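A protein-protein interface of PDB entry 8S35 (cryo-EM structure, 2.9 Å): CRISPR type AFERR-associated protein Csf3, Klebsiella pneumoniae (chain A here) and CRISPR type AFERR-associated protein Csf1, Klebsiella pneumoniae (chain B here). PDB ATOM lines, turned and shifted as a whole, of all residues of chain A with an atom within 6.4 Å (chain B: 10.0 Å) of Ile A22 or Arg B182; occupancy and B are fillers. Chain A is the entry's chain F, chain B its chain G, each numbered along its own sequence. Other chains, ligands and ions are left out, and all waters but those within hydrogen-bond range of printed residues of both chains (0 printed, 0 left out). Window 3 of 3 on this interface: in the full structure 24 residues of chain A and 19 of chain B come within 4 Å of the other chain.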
ATOM      1  N   ILE A  19      25.091  -4.433 -15.202  1.00  0.00           N
ATOM      2  CA  ILE A  19      25.130  -4.589 -16.651  1.00  0.00           C
ATOM      3  C   ILE A  19      26.502  -4.170 -17.153  1.00  0.00           C
ATOM      4  O   ILE A  19      26.972  -3.066 -16.857  1.00  0.00           O
ATOM      5  CB  ILE A  19      24.023  -3.762 -17.324  1.00  0.00           C
ATOM      6  CG1 ILE A  19      22.647  -4.258 -16.866  1.00  0.00           C
ATOM      7  CG2 ILE A  19      24.175  -3.832 -18.844  1.00  0.00           C
ATOM      8  CD1 ILE A  19      21.490  -3.414 -17.340  1.00  0.00           C
ATOM      9  N   SER A  20      27.144  -5.050 -17.916  1.00  0.00           N
ATOM     10  CA  SER A  20      28.473  -4.777 -18.461  1.00  0.00           C
ATOM     11  C   SER A  20      28.359  -4.033 -19.792  1.00  0.00           C
ATOM     12  O   SER A  20      28.792  -4.495 -20.846  1.00  0.00           O
ATOM     13  CB  SER A  20      29.250  -6.078 -18.617  1.00  0.00           C
ATOM     14  OG  SER A  20      29.368  -6.753 -17.380  1.00  0.00           O
ATOM     15  N   GLY A  21      27.752  -2.852 -19.722  1.00  0.00           N
ATOM     16  CA  GLY A  21      27.573  -2.006 -20.885  1.00  0.00           C
ATOM     17  C   GLY A  21      26.486  -2.505 -21.813  1.00  0.00           C
ATOM     18  O   GLY A  21      25.526  -1.785 -22.100  1.00  0.00           O
ATOM     19  N   ILE A  22      26.626  -3.735 -22.283  1.00  0.00           N
ATOM     20  CA  ILE A  22      25.609  -4.399 -23.088  1.00  0.00           C
ATOM     21  C   ILE A  22      24.693  -5.164 -22.151  1.00  0.00           C
ATOM     22  O   ILE A  22      25.159  -5.833 -21.221  1.00  0.00           O
ATOM     23  CB  ILE A  22      26.250  -5.335 -24.129  1.00  0.00           C
ATOM     24  CG1 ILE A  22      27.414  -4.643 -24.845  1.00  0.00           C
ATOM     25  CG2 ILE A  22      25.203  -5.810 -25.126  1.00  0.00           C
ATOM     26  CD1 ILE A  22      27.093  -3.259 -25.373  1.00  0.00           C
ATOM     27  N   ALA A  23      23.390  -5.053 -22.377  1.00  0.00           N
ATOM     28  CA  ALA A  23      22.436  -5.729 -21.514  1.00  0.00           C
ATOM     29  C   ALA A  23      22.697  -7.236 -21.535  1.00  0.00           C
ATOM     30  O   ALA A  23      22.991  -7.794 -22.598  1.00  0.00           O
ATOM     31  CB  ALA A  23      21.007  -5.438 -21.968  1.00  0.00           C
ATOM     32  N   PRO A  24      22.623  -7.924 -20.391  1.00  0.00           N
ATOM     33  CA  PRO A  24      22.861  -9.373 -20.405  1.00  0.00           C
ATOM     34  C   PRO A  24      21.853 -10.095 -21.282  1.00  0.00           C
ATOM     35  O   PRO A  24      20.641  -9.966 -21.104  1.00  0.00           O
ATOM     36  CB  PRO A  24      22.713  -9.775 -18.934  1.00  0.00           C
ATOM     37  CG  PRO A  24      22.946  -8.547 -18.172  1.00  0.00           C
ATOM     38  CD  PRO A  24      22.457  -7.422 -19.016  1.00  0.00           C
ATOM     39  N   SER A  25      22.367 -10.863 -22.235  1.00  0.00           N
ATOM     40  CA  SER A  25      21.529 -11.654 -23.121  1.00  0.00           C
ATOM     41  C   SER A  25      21.237 -13.002 -22.481  1.00  0.00           C
ATOM     42  O   SER A  25      22.128 -13.634 -21.907  1.00  0.00           O
ATOM     43  CB  SER A  25      22.211 -11.853 -24.473  1.00  0.00           C
ATOM     44  OG  SER A  25      21.298 -12.357 -25.431  1.00  0.00           O
ATOM     45  N   SER A  67      17.570  -9.549 -24.972  1.00  0.00           N
ATOM     46  CA  SER A  67      18.394  -9.006 -23.911  1.00  0.00           C
ATOM     47  C   SER A  67      17.561  -8.802 -22.650  1.00  0.00           C
ATOM     48  O   SER A  67      16.334  -8.934 -22.647  1.00  0.00           O
ATOM     49  CB  SER A  67      19.036  -7.688 -24.344  1.00  0.00           C
ATOM     50  OG  SER A  67      20.248  -7.922 -25.037  1.00  0.00           O
ATOM     51  N   PRO A 190      21.813  -8.013 -28.920  1.00  0.00           N
ATOM     52  CA  PRO A 190      22.915  -7.730 -29.849  1.00  0.00           C
ATOM     53  C   PRO A 190      22.707  -8.417 -31.190  1.00  0.00           C
ATOM     54  O   PRO A 190      22.482  -9.627 -31.258  1.00  0.00           O
ATOM     55  CB  PRO A 190      24.143  -8.272 -29.115  1.00  0.00           C
ATOM     56  CG  PRO A 190      23.783  -8.197 -27.685  1.00  0.00           C
ATOM     57  CD  PRO A 190      22.312  -8.465 -27.610  1.00  0.00           C
ATOM     58  N   LYS A 201      24.823   1.490 -31.323  1.00  0.00           N
ATOM     59  CA  LYS A 201      26.022   0.854 -31.842  1.00  0.00           C
ATOM     60  C   LYS A 201      26.902   0.369 -30.699  1.00  0.00           C
ATOM     61  O   LYS A 201      26.929   0.953 -29.612  1.00  0.00           O
ATOM     62  CB  LYS A 201      26.807   1.824 -32.723  1.00  0.00           C
ATOM     63  CG  LYS A 201      26.053   2.302 -33.953  1.00  0.00           C
ATOM     64  CD  LYS A 201      26.032   1.247 -35.043  1.00  0.00           C
ATOM     65  CE  LYS A 201      25.413   1.787 -36.321  1.00  0.00           C
ATOM     66  NZ  LYS A 201      23.988   2.177 -36.131  1.00  0.00           N
ATOM     67  N   GLY A 202      27.623  -0.715 -30.951  1.00  0.00           N
ATOM     68  CA  GLY A 202      28.535  -1.248 -29.960  1.00  0.00           C
ATOM     69  C   GLY A 202      29.475  -2.235 -30.611  1.00  0.00           C
ATOM     70  O   GLY A 202      29.354  -2.554 -31.796  1.00  0.00           O
ATOM     71  N   VAL A 203      30.426  -2.712 -29.815  1.00  0.00           N
ATOM     72  CA  VAL A 203      31.349  -3.760 -30.227  1.00  0.00           C
ATOM     73  C   VAL A 203      31.224  -4.906 -29.231  1.00  0.00           C
ATOM     74  O   VAL A 203      31.306  -4.692 -28.016  1.00  0.00           O
ATOM     75  CB  VAL A 203      32.795  -3.234 -30.323  1.00  0.00           C
ATOM     76  CG1 VAL A 203      33.395  -2.993 -28.942  1.00  0.00           C
ATOM     77  CG2 VAL A 203      33.657  -4.187 -31.134  1.00  0.00           C
ATOM     78  N   SER A 204      30.986  -6.108 -29.740  1.00  0.00           N
ATOM     79  CA  SER A 204      30.830  -7.287 -28.902  1.00  0.00           C
ATOM     80  C   SER A 204      30.738  -8.512 -29.806  1.00  0.00           C
ATOM     81  O   SER A 204      30.344  -8.390 -30.968  1.00  0.00           O
ATOM     82  CB  SER A 204      29.576  -7.186 -28.021  1.00  0.00           C
ATOM     83  OG  SER A 204      29.300  -8.426 -27.396  1.00  0.00           O
ATOM     84  N   TYR A 210      30.496 -13.781 -24.262  1.00  0.00           N
ATOM     85  CA  TYR A 210      30.729 -12.443 -24.780  1.00  0.00           C
ATOM     86  C   TYR A 210      32.092 -11.878 -24.407  1.00  0.00           C
ATOM     87  O   TYR A 210      32.316 -10.680 -24.610  1.00  0.00           O
ATOM     88  CB  TYR A 210      29.618 -11.516 -24.295  1.00  0.00           C
ATOM     89  CG  TYR A 210      28.292 -11.827 -24.940  1.00  0.00           C
ATOM     90  CD1 TYR A 210      28.006 -11.382 -26.219  1.00  0.00           C
ATOM     91  CD2 TYR A 210      27.336 -12.581 -24.279  1.00  0.00           C
ATOM     92  CE1 TYR A 210      26.802 -11.668 -26.819  1.00  0.00           C
ATOM     93  CE2 TYR A 210      26.127 -12.871 -24.872  1.00  0.00           C
ATOM     94  CZ  TYR A 210      25.867 -12.412 -26.143  1.00  0.00           C
ATOM     95  OH  TYR A 210      24.666 -12.695 -26.746  1.00  0.00           O
ATOM     96  N   LYS A 215      35.635  -8.991 -31.469  1.00  0.00           N
ATOM     97  CA  LYS A 215      34.557  -8.055 -31.168  1.00  0.00           C
ATOM     98  C   LYS A 215      34.254  -7.269 -32.434  1.00  0.00           C
ATOM     99  O   LYS A 215      34.966  -6.327 -32.785  1.00  0.00           O
ATOM    100  CB  LYS A 215      34.946  -7.140 -30.012  1.00  0.00           C
ATOM    101  CG  LYS A 215      35.605  -7.859 -28.846  1.00  0.00           C
ATOM    102  CD  LYS A 215      35.761  -6.941 -27.643  1.00  0.00           C
ATOM    103  CE  LYS A 215      34.571  -7.052 -26.702  1.00  0.00           C
ATOM    104  NZ  LYS A 215      34.583  -8.327 -25.934  1.00  0.00           N
ATOM    105  N   ILE A 218      28.199  -4.290 -33.788  1.00  0.00           N
ATOM    106  CA  ILE A 218      26.857  -4.791 -33.526  1.00  0.00           C
ATOM    107  C   ILE A 218      25.930  -3.639 -33.164  1.00  0.00           C
ATOM    108  O   ILE A 218      26.365  -2.538 -32.824  1.00  0.00           O
ATOM    109  CB  ILE A 218      26.865  -5.881 -32.418  1.00  0.00           C
ATOM    110  CG1 ILE A 218      27.120  -5.298 -31.014  1.00  0.00           C
ATOM    111  CG2 ILE A 218      27.853  -6.976 -32.733  1.00  0.00           C
ATOM    112  CD1 ILE A 218      25.963  -4.674 -30.294  1.00  0.00           C
ATOM    113  N   HIS A 220      22.795  -3.084 -30.467  1.00  0.00           N
ATOM    114  CA  HIS A 220      22.190  -3.645 -29.270  1.00  0.00           C
ATOM    115  C   HIS A 220      21.171  -2.676 -28.695  1.00  0.00           C
ATOM    116  O   HIS A 220      21.261  -1.467 -28.922  1.00  0.00           O
ATOM    117  CB  HIS A 220      23.250  -3.954 -28.207  1.00  0.00           C
ATOM    118  CG  HIS A 220      23.844  -2.736 -27.572  1.00  0.00           C
ATOM    119  ND1 HIS A 220      23.335  -2.170 -26.423  1.00  0.00           N
ATOM    120  CD2 HIS A 220      24.911  -1.983 -27.924  1.00  0.00           C
ATOM    121  CE1 HIS A 220      24.061  -1.115 -26.099  1.00  0.00           C
ATOM    122  NE2 HIS A 220      25.025  -0.980 -26.993  1.00  0.00           N
ATOM    123  N   PRO A 221      20.183  -3.179 -27.942  1.00  0.00           N
ATOM    124  CA  PRO A 221      19.174  -2.278 -27.376  1.00  0.00           C
ATOM    125  C   PRO A 221      19.742  -1.414 -26.269  1.00  0.00           C
ATOM    126  O   PRO A 221      20.935  -1.497 -25.956  1.00  0.00           O
ATOM    127  CB  PRO A 221      18.111  -3.239 -26.837  1.00  0.00           C
ATOM    128  CG  PRO A 221      18.859  -4.463 -26.511  1.00  0.00           C
ATOM    129  CD  PRO A 221      19.927  -4.579 -27.556  1.00  0.00           C
ATOM    130  N   PRO A 223      20.914  -0.461 -22.765  1.00  0.00           N
ATOM    131  CA  PRO A 223      21.367  -1.390 -21.715  1.00  0.00           C
ATOM    132  C   PRO A 223      20.333  -1.609 -20.628  1.00  0.00           C
ATOM    133  O   PRO A 223      20.171  -2.739 -20.152  1.00  0.00           O
ATOM    134  CB  PRO A 223      22.630  -0.713 -21.165  1.00  0.00           C
ATOM    135  CG  PRO A 223      23.087   0.182 -22.242  1.00  0.00           C
ATOM    136  CD  PRO A 223      21.861   0.653 -22.943  1.00  0.00           C
ATOM    137  N   ARG B 161      44.076   4.025 -17.809  1.00  0.00           N
ATOM    138  CA  ARG B 161      43.287   2.941 -18.370  1.00  0.00           C
ATOM    139  C   ARG B 161      41.813   3.300 -18.498  1.00  0.00           C
ATOM    140  O   ARG B 161      41.057   2.525 -19.094  1.00  0.00           O
ATOM    141  CB  ARG B 161      43.446   1.685 -17.510  1.00  0.00           C
ATOM    142  CG  ARG B 161      43.632   0.409 -18.312  1.00  0.00           C
ATOM    143  CD  ARG B 161      44.054  -0.757 -17.428  1.00  0.00           C
ATOM    144  NE  ARG B 161      45.485  -0.740 -17.135  1.00  0.00           N
ATOM    145  CZ  ARG B 161      46.043  -0.267 -16.025  1.00  0.00           C
ATOM    146  NH1 ARG B 161      45.322   0.278 -15.057  1.00  0.00           N
ATOM    147  NH2 ARG B 161      47.363  -0.340 -15.884  1.00  0.00           N
ATOM    148  N   SER B 162      41.393   4.449 -17.964  1.00  0.00           N
ATOM    149  CA  SER B 162      40.026   4.928 -18.098  1.00  0.00           C
ATOM    150  C   SER B 162      39.862   6.010 -19.157  1.00  0.00           C
ATOM    151  O   SER B 162      38.726   6.399 -19.447  1.00  0.00           O
ATOM    152  CB  SER B 162      39.529   5.466 -16.753  1.00  0.00           C
ATOM    153  OG  SER B 162      39.193   4.404 -15.879  1.00  0.00           O
ATOM    154  N   ARG B 164      39.187   7.784 -22.495  1.00  0.00           N
ATOM    155  CA  ARG B 164      38.451   7.404 -23.694  1.00  0.00           C
ATOM    156  C   ARG B 164      38.062   8.668 -24.443  1.00  0.00           C
ATOM    157  O   ARG B 164      37.550   9.617 -23.842  1.00  0.00           O
ATOM    158  CB  ARG B 164      37.191   6.596 -23.356  1.00  0.00           C
ATOM    159  CG  ARG B 164      37.428   5.241 -22.698  1.00  0.00           C
ATOM    160  CD  ARG B 164      38.020   4.225 -23.662  1.00  0.00           C
ATOM    161  NE  ARG B 164      38.585   3.078 -22.961  1.00  0.00           N
ATOM    162  CZ  ARG B 164      37.876   2.140 -22.349  1.00  0.00           C
ATOM    163  NH1 ARG B 164      36.552   2.169 -22.335  1.00  0.00           N
ATOM    164  NH2 ARG B 164      38.509   1.146 -21.733  1.00  0.00           N
ATOM    165  N   TYR B 173      32.906  10.835 -22.227  1.00  0.00           N
ATOM    166  CA  TYR B 173      33.430   9.874 -21.262  1.00  0.00           C
ATOM    167  C   TYR B 173      34.261  10.614 -20.221  1.00  0.00           C
ATOM    168  O   TYR B 173      35.327  11.155 -20.532  1.00  0.00           O
ATOM    169  CB  TYR B 173      34.270   8.811 -21.962  1.00  0.00           C
ATOM    170  CG  TYR B 173      33.467   7.852 -22.803  1.00  0.00           C
ATOM    171  CD1 TYR B 173      32.670   6.883 -22.212  1.00  0.00           C
ATOM    172  CD2 TYR B 173      33.506   7.914 -24.186  1.00  0.00           C
ATOM    173  CE1 TYR B 173      31.934   6.004 -22.976  1.00  0.00           C
ATOM    174  CE2 TYR B 173      32.774   7.039 -24.960  1.00  0.00           C
ATOM    175  CZ  TYR B 173      31.990   6.086 -24.349  1.00  0.00           C
ATOM    176  OH  TYR B 173      31.257   5.210 -25.117  1.00  0.00           O
ATOM    177  N   GLN B 178      39.041   6.339 -11.718  1.00  0.00           N
ATOM    178  CA  GLN B 178      38.499   5.034 -11.371  1.00  0.00           C
ATOM    179  C   GLN B 178      38.475   4.182 -12.631  1.00  0.00           C
ATOM    180  O   GLN B 178      38.048   4.654 -13.689  1.00  0.00           O
ATOM    181  CB  GLN B 178      37.091   5.158 -10.790  1.00  0.00           C
ATOM    182  CG  GLN B 178      36.978   6.096  -9.600  1.00  0.00           C
ATOM    183  CD  GLN B 178      37.674   5.561  -8.368  1.00  0.00           C
ATOM    184  OE1 GLN B 178      38.222   4.459  -8.379  1.00  0.00           O
ATOM    185  NE2 GLN B 178      37.657   6.341  -7.293  1.00  0.00           N
ATOM    186  N   LEU B 179      38.948   2.941 -12.519  1.00  0.00           N
ATOM    187  CA  LEU B 179      39.119   2.091 -13.691  1.00  0.00           C
ATOM    188  C   LEU B 179      37.801   1.945 -14.441  1.00  0.00           C
ATOM    189  O   LEU B 179      36.805   1.475 -13.885  1.00  0.00           O
ATOM    190  CB  LEU B 179      39.647   0.721 -13.269  1.00  0.00           C
ATOM    191  CG  LEU B 179      40.337  -0.091 -14.367  1.00  0.00           C
ATOM    192  CD1 LEU B 179      41.519  -0.858 -13.799  1.00  0.00           C
ATOM    193  CD2 LEU B 179      39.360  -1.043 -15.033  1.00  0.00           C
ATOM    194  N   LEU B 180      37.809   2.354 -15.709  1.00  0.00           N
ATOM    195  CA  LEU B 180      36.599   2.420 -16.527  1.00  0.00           C
ATOM    196  C   LEU B 180      36.304   1.042 -17.108  1.00  0.00           C
ATOM    197  O   LEU B 180      36.515   0.766 -18.292  1.00  0.00           O
ATOM    198  CB  LEU B 180      36.763   3.458 -17.629  1.00  0.00           C
ATOM    199  CG  LEU B 180      35.524   3.784 -18.462  1.00  0.00           C
ATOM    200  CD1 LEU B 180      34.481   4.476 -17.613  1.00  0.00           C
ATOM    201  CD2 LEU B 180      35.899   4.644 -19.656  1.00  0.00           C
ATOM    202  N   THR B 181      35.802   0.159 -16.252  1.00  0.00           N
ATOM    203  CA  THR B 181      35.347  -1.133 -16.725  1.00  0.00           C
ATOM    204  C   THR B 181      34.090  -0.957 -17.572  1.00  0.00           C
ATOM    205  O   THR B 181      33.442   0.092 -17.563  1.00  0.00           O
ATOM    206  CB  THR B 181      35.055  -2.069 -15.553  1.00  0.00           C
ATOM    207  OG1 THR B 181      34.010  -1.513 -14.746  1.00  0.00           O
ATOM    208  CG2 THR B 181      36.297  -2.273 -14.702  1.00  0.00           C
ATOM    209  N   ARG B 182      33.741  -2.004 -18.319  1.00  0.00           N
ATOM    210  CA  ARG B 182      32.501  -1.957 -19.079  1.00  0.00           C
ATOM    211  C   ARG B 182      31.270  -1.992 -18.185  1.00  0.00           C
ATOM    212  O   ARG B 182      30.159  -1.781 -18.683  1.00  0.00           O
ATOM    213  CB  ARG B 182      32.444  -3.124 -20.065  1.00  0.00           C
ATOM    214  CG  ARG B 182      33.531  -3.102 -21.134  1.00  0.00           C
ATOM    215  CD  ARG B 182      33.416  -1.902 -22.068  1.00  0.00           C
ATOM    216  NE  ARG B 182      32.068  -1.728 -22.595  1.00  0.00           N
ATOM    217  CZ  ARG B 182      31.493  -2.529 -23.483  1.00  0.00           C
ATOM    218  NH1 ARG B 182      32.124  -3.580 -23.982  1.00  0.00           N
ATOM    219  NH2 ARG B 182      30.252  -2.268 -23.882  1.00  0.00           N
ATOM    220  N   GLN B 183      31.437  -2.252 -16.888  1.00  0.00           N
ATOM    221  CA  GLN B 183      30.322  -2.248 -15.953  1.00  0.00           C
ATOM    222  C   GLN B 183      29.998  -0.871 -15.408  1.00  0.00           C
ATOM    223  O   GLN B 183      28.848  -0.625 -15.029  1.00  0.00           O
ATOM    224  CB  GLN B 183      30.624  -3.170 -14.774  1.00  0.00           C
ATOM    225  CG  GLN B 183      30.685  -4.623 -15.139  1.00  0.00           C
ATOM    226  CD  GLN B 183      32.073  -5.059 -15.550  1.00  0.00           C
ATOM    227  OE1 GLN B 183      33.033  -4.903 -14.796  1.00  0.00           O
ATOM    228  NE2 GLN B 183      32.191  -5.608 -16.752  1.00  0.00           N
ATOM    229  N   ASN B 184      30.971   0.041 -15.383  1.00  0.00           N
ATOM    230  CA  ASN B 184      30.822   1.306 -14.679  1.00  0.00           C
ATOM    231  C   ASN B 184      31.022   2.518 -15.571  1.00  0.00           C
ATOM    232  O   ASN B 184      31.181   3.629 -15.053  1.00  0.00           O
ATOM    233  CB  ASN B 184      31.795   1.368 -13.497  1.00  0.00           C
ATOM    234  CG  ASN B 184      33.240   1.268 -13.927  1.00  0.00           C
ATOM    235  OD1 ASN B 184      33.537   0.992 -15.087  1.00  0.00           O
ATOM    236  ND2 ASN B 184      34.152   1.491 -12.990  1.00  0.00           N
ATOM    237  N   GLU B 185      30.999   2.352 -16.892  1.00  0.00           N
ATOM    238  CA  GLU B 185      31.063   3.530 -17.741  1.00  0.00           C
ATOM    239  C   GLU B 185      29.756   4.308 -17.719  1.00  0.00           C
ATOM    240  O   GLU B 185      29.754   5.493 -18.059  1.00  0.00           O
ATOM    241  CB  GLU B 185      31.436   3.128 -19.175  1.00  0.00           C
ATOM    242  CG  GLU B 185      30.306   2.574 -20.056  1.00  0.00           C
ATOM    243  CD  GLU B 185      29.760   1.245 -19.573  1.00  0.00           C
ATOM    244  OE1 GLU B 185      29.817   0.974 -18.356  1.00  0.00           O
ATOM    245  OE2 GLU B 185      29.276   0.465 -20.418  1.00  0.00           O
ATOM    246  N   VAL B 186      28.658   3.690 -17.274  1.00  0.00           N
ATOM    247  CA  VAL B 186      27.407   4.429 -17.141  1.00  0.00           C
ATOM    248  C   VAL B 186      27.554   5.535 -16.107  1.00  0.00           C
ATOM    249  O   VAL B 186      26.946   6.604 -16.237  1.00  0.00           O
ATOM    250  CB  VAL B 186      26.253   3.464 -16.796  1.00  0.00           C
ATOM    251  CG1 VAL B 186      26.337   3.019 -15.353  1.00  0.00           C
ATOM    252  CG2 VAL B 186      24.910   4.112 -17.089  1.00  0.00           C
ATOM    253  N   LEU B 187      28.364   5.305 -15.072  1.00  0.00           N
ATOM    254  CA  LEU B 187      28.635   6.321 -14.064  1.00  0.00           C
ATOM    255  C   LEU B 187      29.657   7.346 -14.525  1.00  0.00           C
ATOM    256  O   LEU B 187      29.833   8.366 -13.850  1.00  0.00           O
ATOM    257  CB  LEU B 187      29.135   5.664 -12.775  1.00  0.00           C
ATOM    258  CG  LEU B 187      28.136   5.630 -11.620  1.00  0.00           C
ATOM    259  CD1 LEU B 187      26.849   4.943 -12.040  1.00  0.00           C
ATOM    260  CD2 LEU B 187      28.750   4.940 -10.414  1.00  0.00           C
ATOM    261  N   TYR B 188      30.331   7.097 -15.646  1.00  0.00           N
ATOM    262  CA  TYR B 188      31.355   7.983 -16.177  1.00  0.00           C
ATOM    263  C   TYR B 188      31.023   8.470 -17.582  1.00  0.00           C
ATOM    264  O   TYR B 188      31.847   9.149 -18.204  1.00  0.00           O
ATOM    265  CB  TYR B 188      32.708   7.271 -16.149  1.00  0.00           C
ATOM    266  CG  TYR B 188      33.097   6.812 -14.759  1.00  0.00           C
ATOM    267  CD1 TYR B 188      33.095   7.696 -13.689  1.00  0.00           C
ATOM    268  CD2 TYR B 188      33.447   5.495 -14.515  1.00  0.00           C
ATOM    269  CE1 TYR B 188      33.438   7.284 -12.421  1.00  0.00           C
ATOM    270  CE2 TYR B 188      33.792   5.072 -13.247  1.00  0.00           C
ATOM    271  CZ  TYR B 188      33.784   5.972 -12.204  1.00  0.00           C
ATOM    272  OH  TYR B 188      34.125   5.563 -10.936  1.00  0.00           O
ATOM    273  N   MET B 189      29.840   8.138 -18.092  1.00  0.00           N
ATOM    274  CA  MET B 189      29.377   8.566 -19.404  1.00  0.00           C
ATOM    275  C   MET B 189      28.379   9.697 -19.194  1.00  0.00           C
ATOM    276  O   MET B 189      27.418   9.549 -18.431  1.00  0.00           O
ATOM    277  CB  MET B 189      28.782   7.359 -20.146  1.00  0.00           C
ATOM    278  CG  MET B 189      28.457   7.484 -21.629  1.00  0.00           C
ATOM    279  SD  MET B 189      27.650   8.948 -22.291  1.00  0.00           S
ATOM    280  CE  MET B 189      26.096   9.062 -21.396  1.00  0.00           C
ATOM    281  N   ASP B 249      17.668   4.353 -18.061  1.00  0.00           N
ATOM    282  CA  ASP B 249      18.645   3.964 -17.053  1.00  0.00           C
ATOM    283  C   ASP B 249      18.542   4.884 -15.838  1.00  0.00           C
ATOM    284  O   ASP B 249      18.598   6.109 -15.993  1.00  0.00           O
ATOM    285  CB  ASP B 249      20.050   4.018 -17.642  1.00  0.00           C
ATOM    286  CG  ASP B 249      21.093   3.404 -16.731  1.00  0.00           C
ATOM    287  OD1 ASP B 249      21.210   3.841 -15.567  1.00  0.00           O
ATOM    288  OD2 ASP B 249      21.809   2.488 -17.185  1.00  0.00           O
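The backbone NH (N) of Gly A21 sits at hydrogen-bond distance from the backbone carbonyl oxygen (O) of Arg B182, at 2.8 Å.
The side-chain amide nitrogen (NE2) of Gln B183 lies within hydrogen-bond range of the side-chain hydroxyl (OG) of Ser A20, 3.1 Å away.
OG1 of Thr B181 sits close to N of Gln B183, 3.4 Å away.
Ile A19 touches Arg B182.
Gln B183 touches Ile A19 (CA to O, 3.6 Å).
O of Arg B182 touches C of Ser A20, at 3.1 Å.
Gly A21 touches Glu B185.
Ile A22 touches Arg B182.
Of the printed residues of chain A, Arg B182 touches Ile A19, Ser A20, Gly A21 and Ile A22.
Of chain B, only Arg B182 (3.1 Å) and Gln B183 (3.1 Å) come within 4 Å of Ser A20.
Gly A21 touches just these residues of chain B: Arg B182 and Glu B185.
No residue of chain B comes within 4 Å of Ala A23.
Of the printed residues of chain B, Ile A19 touches Arg B182 (3.9 Å) and Gln B183 (3.6 Å).
Printed residues of chain A within 4 Å of Gln B183: Ile A19 (3.6 Å) and Ser A20 (3.1 Å).
Of the printed residues of chain A, Glu B185 touches Gly A21 (3.0 Å).
Of the 19 printed residues of chain A, 4 touch a printed residue of chain B.
Among the printed residues, 7 pairs touch across the chains.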
